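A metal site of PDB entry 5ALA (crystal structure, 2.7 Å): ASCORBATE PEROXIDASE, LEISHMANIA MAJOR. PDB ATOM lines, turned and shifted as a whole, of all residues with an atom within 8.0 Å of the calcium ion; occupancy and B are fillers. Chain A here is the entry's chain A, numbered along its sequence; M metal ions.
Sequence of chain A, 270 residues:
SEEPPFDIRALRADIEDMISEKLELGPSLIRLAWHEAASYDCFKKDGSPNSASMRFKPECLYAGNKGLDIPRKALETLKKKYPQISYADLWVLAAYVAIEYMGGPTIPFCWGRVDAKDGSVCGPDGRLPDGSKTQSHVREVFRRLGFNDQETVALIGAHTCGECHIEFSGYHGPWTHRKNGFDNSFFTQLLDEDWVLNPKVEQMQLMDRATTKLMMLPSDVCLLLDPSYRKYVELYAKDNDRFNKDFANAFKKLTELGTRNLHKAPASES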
ATOM      1  N   LEU A  32       8.865 -34.106  14.108  1.00  0.00           N
ATOM      2  CA  LEU A  32       7.973 -33.117  14.722  1.00  0.00           C
ATOM      3  C   LEU A  32       8.732 -32.138  15.614  1.00  0.00           C
ATOM      4  O   LEU A  32       8.425 -30.951  15.621  1.00  0.00           O
ATOM      5  CB  LEU A  32       6.872 -33.796  15.526  1.00  0.00           C
ATOM      6  CG  LEU A  32       6.009 -32.786  16.291  1.00  0.00           C
ATOM      7  CD1 LEU A  32       5.348 -31.826  15.307  1.00  0.00           C
ATOM      8  CD2 LEU A  32       4.963 -33.450  17.209  1.00  0.00           C
ATOM      9  N   ALA A  33       9.705 -32.616  16.376  1.00  0.00           N
ATOM     10  CA  ALA A  33      10.469 -31.698  17.219  1.00  0.00           C
ATOM     11  C   ALA A  33      11.352 -30.805  16.351  1.00  0.00           C
ATOM     12  O   ALA A  33      11.569 -29.634  16.656  1.00  0.00           O
ATOM     13  CB  ALA A  33      11.312 -32.460  18.220  1.00  0.00           C
ATOM     14  N   TRP A  34      11.830 -31.379  15.242  1.00  0.00           N
ATOM     15  CA  TRP A  34      12.806 -30.703  14.395  1.00  0.00           C
ATOM     16  C   TRP A  34      12.156 -29.594  13.554  1.00  0.00           C
ATOM     17  O   TRP A  34      12.664 -28.485  13.525  1.00  0.00           O
ATOM     18  CB  TRP A  34      13.526 -31.778  13.545  1.00  0.00           C
ATOM     19  CG  TRP A  34      13.690 -31.576  12.064  1.00  0.00           C
ATOM     20  CD1 TRP A  34      13.277 -32.432  11.076  1.00  0.00           C
ATOM     21  CD2 TRP A  34      14.358 -30.493  11.395  1.00  0.00           C
ATOM     22  NE1 TRP A  34      13.624 -31.942   9.837  1.00  0.00           N
ATOM     23  CE2 TRP A  34      14.284 -30.751  10.010  1.00  0.00           C
ATOM     24  CE3 TRP A  34      14.992 -29.335  11.835  1.00  0.00           C
ATOM     25  CZ2 TRP A  34      14.824 -29.886   9.067  1.00  0.00           C
ATOM     26  CZ3 TRP A  34      15.518 -28.474  10.889  1.00  0.00           C
ATOM     27  CH2 TRP A  34      15.440 -28.756   9.520  1.00  0.00           C
ATOM     28  N   HIS A  35      11.015 -29.848  12.948  1.00  0.00           N
ATOM     29  CA  HIS A  35      10.369 -28.795  12.192  1.00  0.00           C
ATOM     30  C   HIS A  35       9.763 -27.735  13.092  1.00  0.00           C
ATOM     31  O   HIS A  35       9.511 -26.619  12.651  1.00  0.00           O
ATOM     32  CB  HIS A  35       9.317 -29.346  11.239  1.00  0.00           C
ATOM     33  CG  HIS A  35       9.894 -29.879   9.968  1.00  0.00           C
ATOM     34  ND1 HIS A  35       9.119 -30.214   8.877  1.00  0.00           N
ATOM     35  CD2 HIS A  35      11.179 -30.129   9.607  1.00  0.00           C
ATOM     36  CE1 HIS A  35       9.908 -30.663   7.910  1.00  0.00           C
ATOM     37  NE2 HIS A  35      11.161 -30.614   8.327  1.00  0.00           N
ATOM     38  N   GLU A  36       9.503 -28.090  14.343  1.00  0.00           N
ATOM     39  CA  GLU A  36       9.089 -27.067  15.304  1.00  0.00           C
ATOM     40  C   GLU A  36      10.199 -26.066  15.544  1.00  0.00           C
ATOM     41  O   GLU A  36       9.935 -24.876  15.693  1.00  0.00           O
ATOM     42  CB  GLU A  36       8.657 -27.706  16.642  1.00  0.00           C
ATOM     43  CG  GLU A  36       8.412 -26.697  17.775  1.00  0.00           C
ATOM     44  CD  GLU A  36       7.403 -25.616  17.418  1.00  0.00           C
ATOM     45  OE1 GLU A  36       6.425 -25.909  16.694  1.00  0.00           O
ATOM     46  OE2 GLU A  36       7.597 -24.459  17.850  1.00  0.00           O
ATOM     47  N   ALA A  37      11.438 -26.536  15.506  1.00  0.00           N
ATOM     48  CA  ALA A  37      12.581 -25.676  15.777  1.00  0.00           C
ATOM     49  C   ALA A  37      13.040 -24.952  14.515  1.00  0.00           C
ATOM     50  O   ALA A  37      13.587 -23.854  14.604  1.00  0.00           O
ATOM     51  CB  ALA A  37      13.713 -26.478  16.354  1.00  0.00           C
ATOM     52  N   ALA A  38      12.773 -25.547  13.350  1.00  0.00           N
ATOM     53  CA  ALA A  38      13.308 -25.081  12.071  1.00  0.00           C
ATOM     54  C   ALA A  38      12.860 -23.704  11.615  1.00  0.00           C
ATOM     55  O   ALA A  38      13.491 -23.128  10.756  1.00  0.00           O
ATOM     56  CB  ALA A  38      12.964 -26.080  10.976  1.00  0.00           C
ATOM     57  N   SER A  39      11.770 -23.174  12.169  1.00  0.00           N
ATOM     58  CA  SER A  39      11.298 -21.851  11.754  1.00  0.00           C
ATOM     59  C   SER A  39      12.277 -20.696  12.092  1.00  0.00           C
ATOM     60  O   SER A  39      12.070 -19.560  11.661  1.00  0.00           O
ATOM     61  CB  SER A  39       9.952 -21.550  12.407  1.00  0.00           C
ATOM     62  OG  SER A  39      10.089 -21.564  13.812  1.00  0.00           O
ATOM     63  N   TYR A  40      13.333 -20.993  12.830  1.00  0.00           N
ATOM     64  CA  TYR A  40      14.209 -19.972  13.399  1.00  0.00           C
ATOM     65  C   TYR A  40      15.100 -19.236  12.381  1.00  0.00           C
ATOM     66  O   TYR A  40      15.727 -19.865  11.527  1.00  0.00           O
ATOM     67  CB  TYR A  40      15.084 -20.641  14.479  1.00  0.00           C
ATOM     68  CG  TYR A  40      15.940 -19.710  15.299  1.00  0.00           C
ATOM     69  CD1 TYR A  40      15.414 -18.574  15.865  1.00  0.00           C
ATOM     70  CD2 TYR A  40      17.272 -20.019  15.564  1.00  0.00           C
ATOM     71  CE1 TYR A  40      16.202 -17.727  16.653  1.00  0.00           C
ATOM     72  CE2 TYR A  40      18.079 -19.181  16.344  1.00  0.00           C
ATOM     73  CZ  TYR A  40      17.535 -18.041  16.886  1.00  0.00           C
ATOM     74  OH  TYR A  40      18.297 -17.202  17.668  1.00  0.00           O
ATOM     75  N   ASP A  46      13.951 -14.425  15.032  1.00  0.00           N
ATOM     76  CA  ASP A  46      12.511 -14.638  15.033  1.00  0.00           C
ATOM     77  C   ASP A  46      12.191 -16.091  14.624  1.00  0.00           C
ATOM     78  O   ASP A  46      13.083 -16.939  14.528  1.00  0.00           O
ATOM     79  CB  ASP A  46      11.825 -13.629  14.101  1.00  0.00           C
ATOM     80  CG  ASP A  46      12.149 -13.875  12.625  1.00  0.00           C
ATOM     81  OD1 ASP A  46      13.262 -14.394  12.332  1.00  0.00           O
ATOM     82  OD2 ASP A  46      11.311 -13.549  11.746  1.00  0.00           O
ATOM     83  N   GLY A  47      10.912 -16.374  14.389  1.00  0.00           N
ATOM     84  CA  GLY A  47      10.494 -17.698  13.958  1.00  0.00           C
ATOM     85  C   GLY A  47       9.799 -18.458  15.070  1.00  0.00           C
ATOM     86  O   GLY A  47       8.963 -19.342  14.832  1.00  0.00           O
ATOM     87  N   SER A  48      10.160 -18.091  16.306  1.00  0.00           N
ATOM     88  CA  SER A  48       9.597 -18.657  17.527  1.00  0.00           C
ATOM     89  C   SER A  48       9.794 -20.169  17.583  1.00  0.00           C
ATOM     90  O   SER A  48       8.829 -20.935  17.653  1.00  0.00           O
ATOM     91  CB  SER A  48       8.116 -18.293  17.642  1.00  0.00           C
ATOM     92  OG  SER A  48       7.630 -18.547  18.945  1.00  0.00           O
ATOM     93  N   PRO A  49      11.066 -20.617  17.573  1.00  0.00           N
ATOM     94  CA  PRO A  49      11.358 -22.052  17.574  1.00  0.00           C
ATOM     95  C   PRO A  49      11.188 -22.670  18.952  1.00  0.00           C
ATOM     96  O   PRO A  49      11.429 -21.990  19.959  1.00  0.00           O
ATOM     97  CB  PRO A  49      12.820 -22.106  17.146  1.00  0.00           C
ATOM     98  CG  PRO A  49      13.395 -20.820  17.734  1.00  0.00           C
ATOM     99  CD  PRO A  49      12.300 -19.797  17.641  1.00  0.00           C
ATOM    100  N   ASN A  50      10.814 -23.948  18.994  1.00  0.00           N
ATOM    101  CA  ASN A  50      10.733 -24.700  20.239  1.00  0.00           C
ATOM    102  C   ASN A  50       9.696 -24.139  21.205  1.00  0.00           C
ATOM    103  O   ASN A  50       9.968 -23.958  22.392  1.00  0.00           O
ATOM    104  CB  ASN A  50      12.124 -24.747  20.904  1.00  0.00           C
ATOM    105  CG  ASN A  50      13.178 -25.442  20.027  1.00  0.00           C
ATOM    106  OD1 ASN A  50      13.010 -26.586  19.632  1.00  0.00           O
ATOM    107  ND2 ASN A  50      14.246 -24.725  19.714  1.00  0.00           N
ATOM    108  N   SER A  51       8.507 -23.830  20.691  1.00  0.00           N
ATOM    109  CA  SER A  51       7.417 -23.312  21.509  1.00  0.00           C
ATOM    110  C   SER A  51       6.117 -24.047  21.215  1.00  0.00           C
ATOM    111  O   SER A  51       5.044 -23.630  21.666  1.00  0.00           O
ATOM    112  CB  SER A  51       7.222 -21.816  21.257  1.00  0.00           C
ATOM    113  OG  SER A  51       6.697 -21.569  19.964  1.00  0.00           O
ATOM    114  N   ALA A  52       6.238 -25.156  20.477  1.00  0.00           N
ATOM    115  CA  ALA A  52       5.100 -25.948  19.991  1.00  0.00           C
ATOM    116  C   ALA A  52       4.104 -25.086  19.230  1.00  0.00           C
ATOM    117  O   ALA A  52       2.887 -25.293  19.334  1.00  0.00           O
ATOM    118  CB  ALA A  52       4.417 -26.662  21.131  1.00  0.00           C
ATOM    119  N   SER A  53       4.611 -24.119  18.478  1.00  0.00           N
ATOM    120  CA  SER A  53       3.763 -23.172  17.755  1.00  0.00           C
ATOM    121  C   SER A  53       3.145 -23.789  16.503  1.00  0.00           C
ATOM    122  O   SER A  53       2.349 -23.147  15.824  1.00  0.00           O
ATOM    123  CB  SER A  53       4.571 -21.928  17.377  1.00  0.00           C
ATOM    124  OG  SER A  53       5.770 -22.286  16.721  1.00  0.00           O
ATOM    125  N   MET A  54       3.513 -25.043  16.233  1.00  0.00           N
ATOM    126  CA  MET A  54       2.940 -25.782  15.108  1.00  0.00           C
ATOM    127  C   MET A  54       1.611 -26.433  15.505  1.00  0.00           C
ATOM    128  O   MET A  54       1.012 -27.189  14.731  1.00  0.00           O
ATOM    129  CB  MET A  54       3.925 -26.864  14.632  1.00  0.00           C
ATOM    130  CG  MET A  54       3.654 -27.429  13.234  1.00  0.00           C
ATOM    131  SD  MET A  54       4.454 -29.034  13.009  1.00  0.00           S
ATOM    132  CE  MET A  54       6.185 -28.573  13.214  1.00  0.00           C
ATOM    133  N   GLU A  59       1.071 -22.433  10.696  1.00  0.00           N
ATOM    134  CA  GLU A  59       2.324 -23.197  10.696  1.00  0.00           C
ATOM    135  C   GLU A  59       2.070 -24.702  10.569  1.00  0.00           C
ATOM    136  O   GLU A  59       2.885 -25.430  10.013  1.00  0.00           O
ATOM    137  CB  GLU A  59       3.137 -22.922  11.961  1.00  0.00           C
ATOM    138  CG  GLU A  59       4.516 -23.546  11.960  1.00  0.00           C
ATOM    139  CD  GLU A  59       5.411 -22.946  13.024  1.00  0.00           C
ATOM    140  OE1 GLU A  59       5.258 -21.735  13.328  1.00  0.00           O
ATOM    141  OE2 GLU A  59       6.257 -23.689  13.567  1.00  0.00           O
ATOM    142  N   TYR A  62       1.484 -25.300   6.839  1.00  0.00           N
ATOM    143  CA  TYR A  62       2.624 -25.163   5.925  1.00  0.00           C
ATOM    144  C   TYR A  62       2.880 -26.445   5.160  1.00  0.00           C
ATOM    145  O   TYR A  62       2.594 -27.544   5.640  1.00  0.00           O
ATOM    146  CB  TYR A  62       3.917 -24.779   6.666  1.00  0.00           C
ATOM    147  CG  TYR A  62       3.978 -23.356   7.168  1.00  0.00           C
ATOM    148  CD1 TYR A  62       2.991 -22.432   6.836  1.00  0.00           C
ATOM    149  CD2 TYR A  62       5.050 -22.927   7.936  1.00  0.00           C
ATOM    150  CE1 TYR A  62       3.058 -21.131   7.294  1.00  0.00           C
ATOM    151  CE2 TYR A  62       5.130 -21.622   8.396  1.00  0.00           C
ATOM    152  CZ  TYR A  62       4.126 -20.726   8.078  1.00  0.00           C
ATOM    153  OH  TYR A  62       4.201 -19.430   8.537  1.00  0.00           O
ATOM    154  N   ASN A  65       5.109 -29.216   6.688  1.00  0.00           N
ATOM    155  CA  ASN A  65       4.742 -29.882   7.932  1.00  0.00           C
ATOM    156  C   ASN A  65       3.593 -30.855   7.770  1.00  0.00           C
ATOM    157  O   ASN A  65       2.892 -31.185   8.739  1.00  0.00           O
ATOM    158  CB  ASN A  65       4.377 -28.852   9.005  1.00  0.00           C
ATOM    159  CG  ASN A  65       5.572 -28.031   9.434  1.00  0.00           C
ATOM    160  OD1 ASN A  65       6.717 -28.480   9.320  1.00  0.00           O
ATOM    161  ND2 ASN A  65       5.314 -26.843   9.942  1.00  0.00           N
ATOM    162  N   TRP A  91       7.125 -32.429  23.066  1.00  0.00           N
ATOM    163  CA  TRP A  91       7.567 -32.730  21.707  1.00  0.00           C
ATOM    164  C   TRP A  91       9.062 -33.048  21.713  1.00  0.00           C
ATOM    165  O   TRP A  91       9.521 -33.959  21.030  1.00  0.00           O
ATOM    166  CB  TRP A  91       7.290 -31.578  20.744  1.00  0.00           C
ATOM    167  CG  TRP A  91       5.841 -31.348  20.500  1.00  0.00           C
ATOM    168  CD1 TRP A  91       4.808 -31.966  21.118  1.00  0.00           C
ATOM    169  CD2 TRP A  91       5.268 -30.425  19.567  1.00  0.00           C
ATOM    170  NE1 TRP A  91       3.608 -31.485  20.643  1.00  0.00           N
ATOM    171  CE2 TRP A  91       3.859 -30.541  19.688  1.00  0.00           C
ATOM    172  CE3 TRP A  91       5.802 -29.504  18.650  1.00  0.00           C
ATOM    173  CZ2 TRP A  91       2.981 -29.776  18.916  1.00  0.00           C
ATOM    174  CZ3 TRP A  91       4.922 -28.741  17.889  1.00  0.00           C
ATOM    175  CH2 TRP A  91       3.531 -28.883  18.029  1.00  0.00           C
ATOM    176  N   VAL A 121       2.282 -15.803  16.831  1.00  0.00           N
ATOM    177  CA  VAL A 121       3.735 -15.705  16.951  1.00  0.00           C
ATOM    178  C   VAL A 121       4.491 -16.598  15.976  1.00  0.00           C
ATOM    179  O   VAL A 121       5.725 -16.585  15.965  1.00  0.00           O
ATOM    180  CB  VAL A 121       4.211 -16.056  18.366  1.00  0.00           C
ATOM    181  CG1 VAL A 121       3.824 -14.960  19.351  1.00  0.00           C
ATOM    182  CG2 VAL A 121       3.651 -17.401  18.797  1.00  0.00           C
ATOM    183  N   CYS A 122       3.768 -17.374  15.177  1.00  0.00           N
ATOM    184  CA  CYS A 122       4.398 -18.315  14.255  1.00  0.00           C
ATOM    185  C   CYS A 122       5.401 -17.626  13.333  1.00  0.00           C
ATOM    186  O   CYS A 122       5.338 -16.419  13.121  1.00  0.00           O
ATOM    187  CB  CYS A 122       3.348 -19.042  13.414  1.00  0.00           C
ATOM    188  SG  CYS A 122       2.210 -20.110  14.337  1.00  0.00           S
ATOM    189  N   GLY A 123       6.322 -18.412  12.779  1.00  0.00           N
ATOM    190  CA  GLY A 123       7.237 -17.870  11.793  1.00  0.00           C
ATOM    191  C   GLY A 123       6.607 -17.884  10.418  1.00  0.00           C
ATOM    192  O   GLY A 123       5.595 -18.548  10.196  1.00  0.00           O
ATOM    193  N   PRO A 124       7.194 -17.117   9.482  1.00  0.00           N
ATOM    194  CA  PRO A 124       6.736 -17.117   8.089  1.00  0.00           C
ATOM    195  C   PRO A 124       6.928 -18.492   7.434  1.00  0.00           C
ATOM    196  O   PRO A 124       7.710 -19.317   7.925  1.00  0.00           O
ATOM    197  CB  PRO A 124       7.632 -16.058   7.439  1.00  0.00           C
ATOM    198  CG  PRO A 124       8.870 -16.084   8.232  1.00  0.00           C
ATOM    199  CD  PRO A 124       8.449 -16.364   9.647  1.00  0.00           C
ATOM    200  N   ARG A 127      10.609 -21.213   5.618  1.00  0.00           N
ATOM    201  CA  ARG A 127      11.778 -21.389   6.473  1.00  0.00           C
ATOM    202  C   ARG A 127      12.297 -22.821   6.422  1.00  0.00           C
ATOM    203  O   ARG A 127      13.509 -23.072   6.508  1.00  0.00           O
ATOM    204  CB  ARG A 127      11.445 -21.003   7.913  1.00  0.00           C
ATOM    205  CG  ARG A 127      11.267 -19.516   8.083  1.00  0.00           C
ATOM    206  CD  ARG A 127      12.586 -18.871   8.471  1.00  0.00           C
ATOM    207  NE  ARG A 127      12.551 -17.423   8.304  1.00  0.00           N
ATOM    208  CZ  ARG A 127      12.177 -16.556   9.243  1.00  0.00           C
ATOM    209  NH1 ARG A 127      11.812 -17.004  10.442  1.00  0.00           N
ATOM    210  NH2 ARG A 127      12.171 -15.256   8.991  1.00  0.00           N
ATOM    211  N   LEU A 128      11.367 -23.759   6.242  1.00  0.00           N
ATOM    212  CA  LEU A 128      11.677 -25.187   6.114  1.00  0.00           C
ATOM    213  C   LEU A 128      12.379 -25.474   4.783  1.00  0.00           C
ATOM    214  O   LEU A 128      12.072 -24.829   3.773  1.00  0.00           O
ATOM    215  CB  LEU A 128      10.389 -26.028   6.219  1.00  0.00           C
ATOM    216  CG  LEU A 128       9.591 -25.856   7.518  1.00  0.00           C
ATOM    217  CD1 LEU A 128       8.194 -26.408   7.373  1.00  0.00           C
ATOM    218  CD2 LEU A 128      10.303 -26.533   8.670  1.00  0.00           C
HETATM  219 CA    CA M   1       8.488 -23.190  14.573  1.00  0.00          CA
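Merely in contact with the calcium ion: Gly 47 (3.9 Å), Ser 48 (3.8 Å) and Ser 53 (3.6 Å).
Six residues have an atom within 4 Å of the calcium ion: Glu 36, Ser 39, Gly 47, Ser 48, Ser 53 and Glu 59.
The nearest printed residue that does not touch the calcium ion is His 35 (4.1 Å).
The side-chain carboxylate (OE2) of Glu 36 lies within hydrogen-bond range of the backbone NH (N) of Asn 50 (3.5 Å).
The backbone carbonyl oxygen of Gly 47 lies within hydrogen-bond range of the backbone NH of Gly 123 (3.5 Å).
The backbone carbonyl oxygen (O) of Ser 39 lies within hydrogen-bond range of the guanidinium group (NH1) of Arg 127 (2.8 Å).
OG of Ser 53 sits at hydrogen-bond distance from OE2 of Glu 36.
The side-chain carboxylate of Glu 36 is in hydrogen-bond range of the backbone NH of Ser 51, at 3.0 Å.
The side-chain carboxylate (OE1) of Glu 59 sits at hydrogen-bond distance from the side-chain hydroxyl (OG) of Ser 53 (3.5 Å).
The backbone NH of Ala 52 is in hydrogen-bond range of the side-chain carboxylate of Glu 36, 3.0 Å away.
The backbone carbonyl oxygen of Ser 53 is in hydrogen-bond range of the side-chain sulfur of Cys 122 (3.4 Å).
The side-chain hydroxyl (OG) of Ser 39 is bound to the calcium ion (2.4 Å).
O of Glu 36 binds the calcium ion (2.5 Å).
The side-chain carboxylate (OE2) of Glu 59 is bound to the calcium ion, at 2.5 Å.
The calcium ion has three donor atoms within binding distance.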
